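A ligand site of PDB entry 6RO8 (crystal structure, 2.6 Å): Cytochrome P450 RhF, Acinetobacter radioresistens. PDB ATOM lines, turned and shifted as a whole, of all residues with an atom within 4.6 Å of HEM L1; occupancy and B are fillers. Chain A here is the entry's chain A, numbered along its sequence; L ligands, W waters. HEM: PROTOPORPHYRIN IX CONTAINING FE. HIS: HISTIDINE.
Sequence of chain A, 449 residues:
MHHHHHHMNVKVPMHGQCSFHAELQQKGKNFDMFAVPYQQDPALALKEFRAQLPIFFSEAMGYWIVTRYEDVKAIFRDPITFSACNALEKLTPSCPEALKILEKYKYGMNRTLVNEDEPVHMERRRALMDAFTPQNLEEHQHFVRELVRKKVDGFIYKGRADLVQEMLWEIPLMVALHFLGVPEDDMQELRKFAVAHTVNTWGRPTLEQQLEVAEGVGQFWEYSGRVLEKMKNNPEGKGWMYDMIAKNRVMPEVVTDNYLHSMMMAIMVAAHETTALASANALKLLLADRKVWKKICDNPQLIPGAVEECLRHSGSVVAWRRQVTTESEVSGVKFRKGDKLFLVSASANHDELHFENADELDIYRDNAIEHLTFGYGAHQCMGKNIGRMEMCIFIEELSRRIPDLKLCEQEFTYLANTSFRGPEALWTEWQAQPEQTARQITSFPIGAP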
ATOM      1  N   PHE A  76      13.119  36.484  23.861  1.00  0.00           N
ATOM      2  CA  PHE A  76      13.473  35.522  24.911  1.00  0.00           C
ATOM      3  C   PHE A  76      14.435  36.139  25.913  1.00  0.00           C
ATOM      4  O   PHE A  76      14.353  35.858  27.121  1.00  0.00           O
ATOM      5  CB  PHE A  76      14.131  34.296  24.296  1.00  0.00           C
ATOM      6  CG  PHE A  76      13.184  33.195  23.977  1.00  0.00           C
ATOM      7  CD1 PHE A  76      12.343  32.674  24.944  1.00  0.00           C
ATOM      8  CD2 PHE A  76      13.161  32.637  22.690  1.00  0.00           C
ATOM      9  CE1 PHE A  76      11.464  31.622  24.647  1.00  0.00           C
ATOM     10  CE2 PHE A  76      12.291  31.580  22.390  1.00  0.00           C
ATOM     11  CZ  PHE A  76      11.444  31.081  23.378  1.00  0.00           C
ATOM     12  N   LEU A 113       7.158  26.983  36.761  1.00  0.00           N
ATOM     13  CA  LEU A 113       8.419  27.609  36.401  1.00  0.00           C
ATOM     14  C   LEU A 113       8.345  28.302  35.060  1.00  0.00           C
ATOM     15  O   LEU A 113       8.772  29.456  34.932  1.00  0.00           O
ATOM     16  CB  LEU A 113       9.540  26.573  36.388  1.00  0.00           C
ATOM     17  CG  LEU A 113      10.133  26.185  37.743  1.00  0.00           C
ATOM     18  CD1 LEU A 113      11.286  25.208  37.555  1.00  0.00           C
ATOM     19  CD2 LEU A 113      10.616  27.424  38.474  1.00  0.00           C
ATOM     20  N   VAL A 114       7.794  27.626  34.039  1.00  0.00           N
ATOM     21  CA  VAL A 114       7.930  28.106  32.676  1.00  0.00           C
ATOM     22  C   VAL A 114       7.118  29.371  32.471  1.00  0.00           C
ATOM     23  O   VAL A 114       7.451  30.183  31.604  1.00  0.00           O
ATOM     24  CB  VAL A 114       7.553  27.001  31.660  1.00  0.00           C
ATOM     25  CG1 VAL A 114       6.035  26.790  31.609  1.00  0.00           C
ATOM     26  CG2 VAL A 114       8.170  27.272  30.266  1.00  0.00           C
ATOM     27  N   MET A 122      10.792  33.632  39.877  1.00  0.00           N
ATOM     28  CA  MET A 122      11.156  32.710  38.811  1.00  0.00           C
ATOM     29  C   MET A 122      12.569  32.148  39.036  1.00  0.00           C
ATOM     30  O   MET A 122      12.751  30.934  39.142  1.00  0.00           O
ATOM     31  CB  MET A 122      11.004  33.446  37.486  1.00  0.00           C
ATOM     32  CG  MET A 122      11.769  32.984  36.293  1.00  0.00           C
ATOM     33  SD  MET A 122      11.919  31.235  35.944  1.00  0.00           S
ATOM     34  CE  MET A 122      13.500  31.276  35.132  1.00  0.00           C
ATOM     35  N   ARG A 126      13.821  28.629  40.410  1.00  0.00           N
ATOM     36  CA  ARG A 126      14.721  27.850  39.563  1.00  0.00           C
ATOM     37  C   ARG A 126      16.054  27.618  40.263  1.00  0.00           C
ATOM     38  O   ARG A 126      16.462  26.463  40.463  1.00  0.00           O
ATOM     39  CB  ARG A 126      14.937  28.554  38.225  1.00  0.00           C
ATOM     40  CG  ARG A 126      15.916  27.802  37.325  1.00  0.00           C
ATOM     41  CD  ARG A 126      15.942  28.311  35.900  1.00  0.00           C
ATOM     42  NE  ARG A 126      16.844  27.496  35.082  1.00  0.00           N
ATOM     43  CZ  ARG A 126      16.721  27.307  33.757  1.00  0.00           C
ATOM     44  NH1 ARG A 126      15.734  27.890  33.078  1.00  0.00           N
ATOM     45  NH2 ARG A 126      17.605  26.544  33.124  1.00  0.00           N
ATOM     46  N   PHE A 179      12.091  10.080  36.865  1.00  0.00           N
ATOM     47  CA  PHE A 179      12.817  11.296  37.223  1.00  0.00           C
ATOM     48  C   PHE A 179      12.088  12.078  38.299  1.00  0.00           C
ATOM     49  O   PHE A 179      12.693  12.497  39.288  1.00  0.00           O
ATOM     50  CB  PHE A 179      13.023  12.149  35.976  1.00  0.00           C
ATOM     51  CG  PHE A 179      13.751  13.433  36.231  1.00  0.00           C
ATOM     52  CD1 PHE A 179      15.124  13.433  36.465  1.00  0.00           C
ATOM     53  CD2 PHE A 179      13.066  14.643  36.216  1.00  0.00           C
ATOM     54  CE1 PHE A 179      15.808  14.631  36.692  1.00  0.00           C
ATOM     55  CE2 PHE A 179      13.733  15.825  36.449  1.00  0.00           C
ATOM     56  CZ  PHE A 179      15.106  15.825  36.683  1.00  0.00           C
ATOM     57  N   TRP A 240      12.494  14.474  41.452  1.00  0.00           N
ATOM     58  CA  TRP A 240      12.475  15.933  41.411  1.00  0.00           C
ATOM     59  C   TRP A 240      11.296  16.520  42.184  1.00  0.00           C
ATOM     60  O   TRP A 240      11.437  17.557  42.844  1.00  0.00           O
ATOM     61  CB  TRP A 240      12.437  16.402  39.967  1.00  0.00           C
ATOM     62  CG  TRP A 240      12.794  17.820  39.844  1.00  0.00           C
ATOM     63  CD1 TRP A 240      13.646  18.536  40.638  1.00  0.00           C
ATOM     64  CD2 TRP A 240      12.334  18.713  38.834  1.00  0.00           C
ATOM     65  NE1 TRP A 240      13.746  19.826  40.193  1.00  0.00           N
ATOM     66  CE2 TRP A 240      12.946  19.963  39.078  1.00  0.00           C
ATOM     67  CE3 TRP A 240      11.473  18.583  37.751  1.00  0.00           C
ATOM     68  CZ2 TRP A 240      12.716  21.073  38.277  1.00  0.00           C
ATOM     69  CZ3 TRP A 240      11.226  19.678  36.957  1.00  0.00           C
ATOM     70  CH2 TRP A 240      11.852  20.903  37.212  1.00  0.00           C
ATOM     71  N   MET A 263       2.814  22.775  39.426  1.00  0.00           N
ATOM     72  CA  MET A 263       3.948  22.146  38.761  1.00  0.00           C
ATOM     73  C   MET A 263       3.726  20.647  38.598  1.00  0.00           C
ATOM     74  O   MET A 263       4.061  20.079  37.556  1.00  0.00           O
ATOM     75  CB  MET A 263       5.249  22.442  39.520  1.00  0.00           C
ATOM     76  CG  MET A 263       6.530  21.941  38.812  1.00  0.00           C
ATOM     77  SD  MET A 263       6.777  22.702  37.190  1.00  0.00           S
ATOM     78  CE  MET A 263       8.508  23.102  37.225  1.00  0.00           C
ATOM     79  N   ILE A 267       4.286  19.617  34.969  1.00  0.00           N
ATOM     80  CA  ILE A 267       5.526  18.884  34.726  1.00  0.00           C
ATOM     81  C   ILE A 267       5.242  17.439  34.322  1.00  0.00           C
ATOM     82  O   ILE A 267       6.049  16.822  33.615  1.00  0.00           O
ATOM     83  CB  ILE A 267       6.476  18.985  35.949  1.00  0.00           C
ATOM     84  CG1 ILE A 267       7.930  18.916  35.465  1.00  0.00           C
ATOM     85  CG2 ILE A 267       6.183  17.899  36.985  1.00  0.00           C
ATOM     86  CD1 ILE A 267       8.242  19.874  34.334  1.00  0.00           C
ATOM     87  N   ALA A 270       5.117  17.971  30.611  1.00  0.00           N
ATOM     88  CA  ALA A 270       6.299  18.554  30.006  1.00  0.00           C
ATOM     89  C   ALA A 270       7.548  17.673  30.136  1.00  0.00           C
ATOM     90  O   ALA A 270       8.416  17.719  29.260  1.00  0.00           O
ATOM     91  CB  ALA A 270       6.560  19.933  30.624  1.00  0.00           C
ATOM     92  N   ALA A 271       7.635  16.834  31.179  1.00  0.00           N
ATOM     93  CA  ALA A 271       8.816  15.994  31.356  1.00  0.00           C
ATOM     94  C   ALA A 271       8.904  14.846  30.353  1.00  0.00           C
ATOM     95  O   ALA A 271       9.868  14.072  30.409  1.00  0.00           O
ATOM     96  CB  ALA A 271       8.870  15.433  32.783  1.00  0.00           C
ATOM     97  N   HIS A 272       7.946  14.712  29.443  1.00  0.00           N
ATOM     98  CA  HIS A 272       8.048  13.573  28.540  1.00  0.00           C
ATOM     99  C   HIS A 272       7.453  13.858  27.167  1.00  0.00           C
ATOM    100  O   HIS A 272       7.995  13.392  26.162  1.00  0.00           O
ATOM    101  CB  HIS A 272       7.401  12.338  29.171  1.00  0.00           C
ATOM    102  CG  HIS A 272       5.908  12.388  29.208  1.00  0.00           C
ATOM    103  ND1 HIS A 272       5.124  11.793  28.247  1.00  0.00           N
ATOM    104  CD2 HIS A 272       5.060  12.951  30.094  1.00  0.00           C
ATOM    105  CE1 HIS A 272       3.856  12.005  28.526  1.00  0.00           C
ATOM    106  NE2 HIS A 272       3.781  12.700  29.652  1.00  0.00           N
ATOM    107  N   THR A 274       7.195  16.445  25.047  1.00  0.00           N
ATOM    108  CA  THR A 274       8.035  17.049  24.015  1.00  0.00           C
ATOM    109  C   THR A 274       9.198  16.134  23.613  1.00  0.00           C
ATOM    110  O   THR A 274       9.639  16.170  22.460  1.00  0.00           O
ATOM    111  CB  THR A 274       8.568  18.415  24.477  1.00  0.00           C
ATOM    112  OG1 THR A 274       8.864  18.398  25.873  1.00  0.00           O
ATOM    113  CG2 THR A 274       7.579  19.516  24.175  1.00  0.00           C
ATOM    114  N   THR A 275       9.709  15.317  24.549  1.00  0.00           N
ATOM    115  CA  THR A 275      10.732  14.329  24.232  1.00  0.00           C
ATOM    116  C   THR A 275      10.203  13.248  23.287  1.00  0.00           C
ATOM    117  O   THR A 275      10.932  12.802  22.386  1.00  0.00           O
ATOM    118  CB  THR A 275      11.270  13.706  25.512  1.00  0.00           C
ATOM    119  OG1 THR A 275      11.712  14.753  26.389  1.00  0.00           O
ATOM    120  CG2 THR A 275      12.455  12.797  25.239  1.00  0.00           C
ATOM    121  N   ALA A 278       9.635  14.921  19.797  1.00  0.00           N
ATOM    122  CA  ALA A 278      10.908  15.246  19.166  1.00  0.00           C
ATOM    123  C   ALA A 278      11.606  13.984  18.661  1.00  0.00           C
ATOM    124  O   ALA A 278      12.194  13.995  17.567  1.00  0.00           O
ATOM    125  CB  ALA A 278      11.827  15.995  20.149  1.00  0.00           C
ATOM    126  N   LEU A 311      16.483  18.778  16.249  1.00  0.00           N
ATOM    127  CA  LEU A 311      15.834  19.744  17.128  1.00  0.00           C
ATOM    128  C   LEU A 311      15.716  21.128  16.476  1.00  0.00           C
ATOM    129  O   LEU A 311      14.715  21.839  16.659  1.00  0.00           O
ATOM    130  CB  LEU A 311      16.632  19.846  18.424  1.00  0.00           C
ATOM    131  CG  LEU A 311      16.506  18.623  19.364  1.00  0.00           C
ATOM    132  CD1 LEU A 311      17.428  18.775  20.599  1.00  0.00           C
ATOM    133  CD2 LEU A 311      15.041  18.427  19.777  1.00  0.00           C
ATOM    134  N   SER A 316      10.121  19.689  18.509  1.00  0.00           N
ATOM    135  CA  SER A 316       8.797  19.359  19.025  1.00  0.00           C
ATOM    136  C   SER A 316       8.049  20.564  19.578  1.00  0.00           C
ATOM    137  O   SER A 316       6.823  20.500  19.679  1.00  0.00           O
ATOM    138  CB  SER A 316       8.896  18.289  20.117  1.00  0.00           C
ATOM    139  OG  SER A 316       9.887  18.658  21.072  1.00  0.00           O
ATOM    140  N   VAL A 317       8.753  21.618  19.951  1.00  0.00           N
ATOM    141  CA  VAL A 317       8.148  22.926  20.202  1.00  0.00           C
ATOM    142  C   VAL A 317       8.391  23.807  18.984  1.00  0.00           C
ATOM    143  O   VAL A 317       9.538  24.098  18.636  1.00  0.00           O
ATOM    144  CB  VAL A 317       8.710  23.577  21.472  1.00  0.00           C
ATOM    145  CG1 VAL A 317       8.109  24.979  21.652  1.00  0.00           C
ATOM    146  CG2 VAL A 317       8.423  22.697  22.696  1.00  0.00           C
ATOM    147  N   TRP A 320       6.299  29.302  20.942  1.00  0.00           N
ATOM    148  CA  TRP A 320       6.089  29.588  22.355  1.00  0.00           C
ATOM    149  C   TRP A 320       5.577  31.037  22.478  1.00  0.00           C
ATOM    150  O   TRP A 320       5.518  31.776  21.500  1.00  0.00           O
ATOM    151  CB  TRP A 320       7.388  29.349  23.143  1.00  0.00           C
ATOM    152  CG  TRP A 320       7.165  28.840  24.537  1.00  0.00           C
ATOM    153  CD1 TRP A 320       7.618  29.424  25.696  1.00  0.00           C
ATOM    154  CD2 TRP A 320       6.457  27.656  24.936  1.00  0.00           C
ATOM    155  NE1 TRP A 320       7.220  28.680  26.792  1.00  0.00           N
ATOM    156  CE2 TRP A 320       6.502  27.594  26.355  1.00  0.00           C
ATOM    157  CE3 TRP A 320       5.762  26.662  24.240  1.00  0.00           C
ATOM    158  CZ2 TRP A 320       5.898  26.559  27.080  1.00  0.00           C
ATOM    159  CZ3 TRP A 320       5.144  25.647  24.964  1.00  0.00           C
ATOM    160  CH2 TRP A 320       5.238  25.596  26.371  1.00  0.00           C
ATOM    161  N   ARG A 322       4.779  34.890  24.672  1.00  0.00           N
ATOM    162  CA  ARG A 322       5.174  35.926  25.605  1.00  0.00           C
ATOM    163  C   ARG A 322       4.042  36.926  25.713  1.00  0.00           C
ATOM    164  O   ARG A 322       3.205  37.046  24.801  1.00  0.00           O
ATOM    165  CB  ARG A 322       6.479  36.629  25.183  1.00  0.00           C
ATOM    166  CG  ARG A 322       7.734  35.814  25.404  1.00  0.00           C
ATOM    167  CD  ARG A 322       7.817  35.398  26.863  1.00  0.00           C
ATOM    168  NE  ARG A 322       9.097  34.767  27.185  1.00  0.00           N
ATOM    169  CZ  ARG A 322       9.262  33.456  27.396  1.00  0.00           C
ATOM    170  NH1 ARG A 322       8.227  32.644  27.310  1.00  0.00           N
ATOM    171  NH2 ARG A 322      10.456  32.983  27.704  1.00  0.00           N
ATOM    172  N   THR A 373      14.628  25.827  19.869  1.00  0.00           N
ATOM    173  CA  THR A 373      13.597  24.890  20.285  1.00  0.00           C
ATOM    174  C   THR A 373      13.545  24.759  21.808  1.00  0.00           C
ATOM    175  O   THR A 373      12.469  24.490  22.372  1.00  0.00           O
ATOM    176  CB  THR A 373      13.840  23.514  19.618  1.00  0.00           C
ATOM    177  OG1 THR A 373      13.925  23.665  18.197  1.00  0.00           O
ATOM    178  CG2 THR A 373      12.746  22.505  19.883  1.00  0.00           C
ATOM    179  N   PHE A 374      14.653  24.979  22.496  1.00  0.00           N
ATOM    180  CA  PHE A 374      14.655  24.917  23.963  1.00  0.00           C
ATOM    181  C   PHE A 374      14.455  26.271  24.617  1.00  0.00           C
ATOM    182  O   PHE A 374      14.553  26.382  25.849  1.00  0.00           O
ATOM    183  CB  PHE A 374      15.964  24.301  24.493  1.00  0.00           C
ATOM    184  CG  PHE A 374      16.108  22.823  24.230  1.00  0.00           C
ATOM    185  CD1 PHE A 374      15.114  21.939  24.597  1.00  0.00           C
ATOM    186  CD2 PHE A 374      17.241  22.334  23.588  1.00  0.00           C
ATOM    187  CE1 PHE A 374      15.249  20.576  24.337  1.00  0.00           C
ATOM    188  CE2 PHE A 374      17.395  20.982  23.330  1.00  0.00           C
ATOM    189  CZ  PHE A 374      16.402  20.095  23.706  1.00  0.00           C
ATOM    190  N   GLY A 375      14.159  27.301  23.814  1.00  0.00           N
ATOM    191  CA  GLY A 375      14.174  28.659  24.292  1.00  0.00           C
ATOM    192  C   GLY A 375      15.590  29.200  24.431  1.00  0.00           C
ATOM    193  O   GLY A 375      16.572  28.627  23.968  1.00  0.00           O
ATOM    194  N   TYR A 376      15.665  30.350  25.101  1.00  0.00           N
ATOM    195  CA  TYR A 376      16.922  31.051  25.290  1.00  0.00           C
ATOM    196  C   TYR A 376      16.771  31.927  26.539  1.00  0.00           C
ATOM    197  O   TYR A 376      15.703  32.506  26.765  1.00  0.00           O
ATOM    198  CB  TYR A 376      17.283  31.899  24.055  1.00  0.00           C
ATOM    199  CG  TYR A 376      18.578  32.670  24.137  1.00  0.00           C
ATOM    200  CD1 TYR A 376      19.774  32.095  23.756  1.00  0.00           C
ATOM    201  CD2 TYR A 376      18.596  33.989  24.578  1.00  0.00           C
ATOM    202  CE1 TYR A 376      20.969  32.803  23.814  1.00  0.00           C
ATOM    203  CE2 TYR A 376      19.793  34.718  24.644  1.00  0.00           C
ATOM    204  CZ  TYR A 376      20.983  34.110  24.262  1.00  0.00           C
ATOM    205  OH  TYR A 376      22.178  34.818  24.320  1.00  0.00           O
ATOM    206  N   ALA A 378      16.331  33.148  30.369  1.00  0.00           N
ATOM    207  CA  ALA A 378      15.926  32.906  31.750  1.00  0.00           C
ATOM    208  C   ALA A 378      15.174  31.599  31.889  1.00  0.00           C
ATOM    209  O   ALA A 378      15.450  30.813  32.812  1.00  0.00           O
ATOM    210  CB  ALA A 378      15.076  34.079  32.260  1.00  0.00           C
ATOM    211  N   HIS A 379      14.232  31.321  30.975  1.00  0.00           N
ATOM    212  CA  HIS A 379      13.357  30.164  31.036  1.00  0.00           C
ATOM    213  C   HIS A 379      13.853  29.008  30.176  1.00  0.00           C
ATOM    214  O   HIS A 379      13.111  28.027  29.999  1.00  0.00           O
ATOM    215  CB  HIS A 379      11.939  30.541  30.631  1.00  0.00           C
ATOM    216  CG  HIS A 379      11.219  31.420  31.615  1.00  0.00           C
ATOM    217  ND1 HIS A 379      10.460  30.925  32.647  1.00  0.00           N
ATOM    218  CD2 HIS A 379      11.158  32.773  31.721  1.00  0.00           C
ATOM    219  CE1 HIS A 379       9.960  31.926  33.349  1.00  0.00           C
ATOM    220  NE2 HIS A 379      10.374  33.050  32.800  1.00  0.00           N
ATOM    221  N   GLN A 380      15.078  29.079  29.667  1.00  0.00           N
ATOM    222  CA  GLN A 380      15.591  28.024  28.802  1.00  0.00           C
ATOM    223  C   GLN A 380      15.427  26.652  29.439  1.00  0.00           C
ATOM    224  O   GLN A 380      15.685  26.466  30.632  1.00  0.00           O
ATOM    225  CB  GLN A 380      17.048  28.249  28.466  1.00  0.00           C
ATOM    226  CG  GLN A 380      17.481  27.288  27.387  1.00  0.00           C
ATOM    227  CD  GLN A 380      18.959  27.153  27.296  1.00  0.00           C
ATOM    228  OE1 GLN A 380      19.620  26.650  28.219  1.00  0.00           O
ATOM    229  NE2 GLN A 380      19.517  27.575  26.163  1.00  0.00           N
ATOM    230  N   CYS A 381      14.998  25.698  28.629  1.00  0.00           N
ATOM    231  CA  CYS A 381      14.482  24.429  29.101  1.00  0.00           C
ATOM    232  C   CYS A 381      15.442  23.744  30.078  1.00  0.00           C
ATOM    233  O   CYS A 381      16.614  23.508  29.758  1.00  0.00           O
ATOM    234  CB  CYS A 381      14.233  23.519  27.908  1.00  0.00           C
ATOM    235  SG  CYS A 381      13.924  21.893  28.474  1.00  0.00           S
ATOM    236  N   MET A 382      14.940  23.417  31.265  1.00  0.00           N
ATOM    237  CA  MET A 382      15.800  22.777  32.261  1.00  0.00           C
ATOM    238  C   MET A 382      16.072  21.314  31.967  1.00  0.00           C
ATOM    239  O   MET A 382      17.062  20.766  32.454  1.00  0.00           O
ATOM    240  CB  MET A 382      15.185  22.882  33.663  1.00  0.00           C
ATOM    241  CG  MET A 382      15.421  24.222  34.301  1.00  0.00           C
ATOM    242  SD  MET A 382      14.569  24.371  35.879  1.00  0.00           S
ATOM    243  CE  MET A 382      15.746  23.653  37.034  1.00  0.00           C
ATOM    244  N   GLY A 383      15.221  20.675  31.159  1.00  0.00           N
ATOM    245  CA  GLY A 383      15.349  19.258  30.889  1.00  0.00           C
ATOM    246  C   GLY A 383      15.908  18.985  29.514  1.00  0.00           C
ATOM    247  O   GLY A 383      15.811  17.845  29.013  1.00  0.00           O
ATOM    248  N   ILE A 386      17.999  15.906  29.328  1.00  0.00           N
ATOM    249  CA  ILE A 386      17.230  14.657  29.395  1.00  0.00           C
ATOM    250  C   ILE A 386      16.620  14.374  28.027  1.00  0.00           C
ATOM    251  O   ILE A 386      16.715  13.255  27.500  1.00  0.00           O
ATOM    252  CB  ILE A 386      16.154  14.743  30.499  1.00  0.00           C
ATOM    253  CG1 ILE A 386      16.814  14.845  31.876  1.00  0.00           C
ATOM    254  CG2 ILE A 386      15.239  13.539  30.406  1.00  0.00           C
ATOM    255  CD1 ILE A 386      15.873  15.438  32.968  1.00  0.00           C
ATOM    256  N   GLY A 387      16.028  15.398  27.409  1.00  0.00           N
ATOM    257  CA  GLY A 387      15.475  15.229  26.068  1.00  0.00           C
ATOM    258  C   GLY A 387      16.508  14.760  25.057  1.00  0.00           C
ATOM    259  O   GLY A 387      16.225  13.863  24.241  1.00  0.00           O
HETATM  260  CHA HEM L   1      11.234  25.152  29.560  1.00  0.00           C
HETATM  261  CHB HEM L   1      11.103  22.840  25.283  1.00  0.00           C
HETATM  262  CHC HEM L   1      11.845  18.541  27.472  1.00  0.00           C
HETATM  263  CHD HEM L   1      11.486  20.846  31.741  1.00  0.00           C
HETATM  264  C1A HEM L   1      11.116  24.917  28.217  1.00  0.00           C
HETATM  265  C2A HEM L   1      10.839  25.888  27.173  1.00  0.00           C
HETATM  266  C3A HEM L   1      10.816  25.255  26.007  1.00  0.00           C
HETATM  267  C4A HEM L   1      11.052  23.845  26.236  1.00  0.00           C
HETATM  268  CMA HEM L   1      10.548  25.931  24.640  1.00  0.00           C
HETATM  269  CAA HEM L   1      10.646  27.405  27.370  1.00  0.00           C
HETATM  270  CBA HEM L   1      11.970  28.077  27.053  1.00  0.00           C
HETATM  271  CGA HEM L   1      11.913  29.556  27.295  1.00  0.00           C
HETATM  272  O1A HEM L   1      10.841  30.078  27.673  1.00  0.00           O
HETATM  273  O2A HEM L   1      12.972  30.209  27.100  1.00  0.00           O
HETATM  274  C1B HEM L   1      11.384  21.505  25.492  1.00  0.00           C
HETATM  275  C2B HEM L   1      11.647  20.526  24.460  1.00  0.00           C
HETATM  276  C3B HEM L   1      11.837  19.334  25.060  1.00  0.00           C
HETATM  277  C4B HEM L   1      11.705  19.524  26.503  1.00  0.00           C
HETATM  278  CMB HEM L   1      11.685  20.871  22.947  1.00  0.00           C
HETATM  279  CAB HEM L   1      12.192  17.954  24.453  1.00  0.00           C
HETATM  280  CBB HEM L   1      12.560  17.741  23.190  1.00  0.00           C
HETATM  281  C1C HEM L   1      11.808  18.781  28.836  1.00  0.00           C
HETATM  282  C2C HEM L   1      11.944  17.816  29.911  1.00  0.00           C
HETATM  283  C3C HEM L   1      11.834  18.482  31.083  1.00  0.00           C
HETATM  284  C4C HEM L   1      11.646  19.871  30.787  1.00  0.00           C
HETATM  285  CMC HEM L   1      12.164  16.304  29.679  1.00  0.00           C
HETATM  286  CAC HEM L   1      11.897  18.002  32.552  1.00  0.00           C
HETATM  287  CBC HEM L   1      12.035  16.715  32.895  1.00  0.00           C
HETATM  288  C1D HEM L   1      11.355  22.193  31.540  1.00  0.00           C
HETATM  289  C2D HEM L   1      11.220  23.189  32.574  1.00  0.00           C
HETATM  290  C3D HEM L   1      11.163  24.378  31.989  1.00  0.00           C
HETATM  291  C4D HEM L   1      11.258  24.188  30.541  1.00  0.00           C
HETATM  292  CMD HEM L   1      11.141  22.940  34.097  1.00  0.00           C
HETATM  293  CAD HEM L   1      10.975  25.716  32.743  1.00  0.00           C
HETATM  294  CBD HEM L   1      12.306  26.320  33.166  1.00  0.00           C
HETATM  295  CGD HEM L   1      12.112  27.794  33.466  1.00  0.00           C
HETATM  296  O1D HEM L   1      10.966  28.264  33.345  1.00  0.00           O
HETATM  297  O2D HEM L   1      13.092  28.498  33.809  1.00  0.00           O
HETATM  298  NA  HEM L   1      11.213  23.675  27.609  1.00  0.00           N
HETATM  299  NB  HEM L   1      11.423  20.857  26.725  1.00  0.00           N
HETATM  300  NC  HEM L   1      11.629  20.024  29.411  1.00  0.00           N
HETATM  301  ND  HEM L   1      11.385  22.831  30.317  1.00  0.00           N
HETATM  302 FE   HEM L   1      11.427  21.815  28.528  1.00  0.00          FE
HETATM  303  N   HIS L   2       5.028  21.867  28.044  1.00  0.00           N
HETATM  304  CA  HIS L   2       6.233  22.217  27.312  1.00  0.00           C
HETATM  305  C   HIS L   2       7.179  21.033  27.187  1.00  0.00           C
HETATM  306  O   HIS L   2       8.301  21.190  26.692  1.00  0.00           O
HETATM  307  CB  HIS L   2       6.955  23.385  27.987  1.00  0.00           C
HETATM  308  CG  HIS L   2       6.969  23.304  29.489  1.00  0.00           C
HETATM  309  ND1 HIS L   2       8.130  23.415  30.225  1.00  0.00           N
HETATM  310  CD2 HIS L   2       5.972  23.115  30.378  1.00  0.00           C
HETATM  311  CE1 HIS L   2       7.838  23.291  31.509  1.00  0.00           C
HETATM  312  NE2 HIS L   2       6.533  23.111  31.628  1.00  0.00           N
HETATM  313  OXT HIS L   2       6.836  19.906  27.564  1.00  0.00           O
HETATM  314  O   HOH W   1       9.790  16.042  27.322  1.00  0.00           O
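SD of Met 122 lies close to O2D of HEM L1 (3.7 Å). O of Ala 378 lies close to O2D of HEM L1 (3.5 Å). Phe 76 touches HEM L1 (CE1 to O2A, 3.2 Å). Trp 240 touches HEM L1. Ala 270 touches HEM L1. O of Ala 271 touches CMC of HEM L1 (3.3 Å). OG1 of Thr 274 touches C4B of HEM L1, at 3.1 Å. N of Thr 275 touches CAB of HEM L1, 3.6 Å away. Ala 278 touches HEM L1. Ser 316 touches HEM L1. CG2 of Val 317 touches CHB of HEM L1, 3.7 Å away. Trp 320 touches HEM L1. O of Thr 373 touches CMA of HEM L1 (3.3 Å). O of Phe 374 touches CBA of HEM L1, 3.3 Å away. CA of Gly 375 touches O2A of HEM L1 (3.4 Å). N of Gln 380 touches O2A of HEM L1, 3.5 Å away. N of Met 382 touches ND of HEM L1, 3.7 Å away. CA of Gly 383 touches C3C of HEM L1 (3.6 Å). The nearest printed residue that does not touch HEM L1 is Phe 179 (4.04 Å).
SG of Cys 381 is bound to FE of HEM L1 (2.5 Å). ND1 of His 379 lies within hydrogen-bond range of O1D of HEM L1 (2.8 Å). An oxygen (O2D) of HEM L1 is in salt-bridge range of the guanidinium group (NH1) of Arg 126 (2.8 Å). The guanidinium group (NH2) of Arg 322 lies within salt-bridge range of an oxygen (O1A) of HEM L1 (2.9 Å). The backbone carbonyl oxygen of Leu 113 lies close to an oxygen (O1D) of HEM L1, at 3.0 Å. The backbone NH (N) of Val 114 lies close to an oxygen (O1D) of HEM L1, at 3.3 Å. An oxygen (O2A) of HEM L1 is in hydrogen-bond range of the backbone NH (N) of Tyr 376. The side-chain hydroxyl (OG1) of Thr 274 is in hydrogen-bond range of an oxygen (O) of HIS L2, at 3.0 Å.
The backbone NH of Cys 381 lies within hydrogen-bond range of the backbone carbonyl oxygen of Phe 374 (2.9 Å). SG of Cys 381 sits close to N of Gly 383 (3.2 Å). A ring nitrogen (ND1) of His 379 lies close to the backbone carbonyl oxygen (O) of Leu 113, at 3.2 Å. ND1 of His 379 is in hydrogen-bond range of O of Val 114 (3.3 Å). The guanidinium group (NH1) of Arg 126 is in hydrogen-bond range of the backbone carbonyl oxygen (O) of Ala 378 (2.9 Å). The backbone carbonyl oxygen of Thr 274 sits at hydrogen-bond distance from the side-chain hydroxyl of Ser 316 (2.9 Å). The side-chain hydroxyl (OG1) of Thr 373 lies within hydrogen-bond range of the backbone carbonyl oxygen (O) of Leu 311 (2.5 Å). O of Phe 179 sits at hydrogen-bond distance from N of Trp 240 (2.9 Å).
Water W1 lies within hydrogen-bond range of the side-chain hydroxyl (OG1) of Thr 275 (2.5 Å), the backbone carbonyl oxygen (O) of Ala 270 (2.9 Å), the side-chain hydroxyl (OG1) of Thr 274 (2.9 Å) and the backbone NH (N) of His 272 (3.1 Å).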
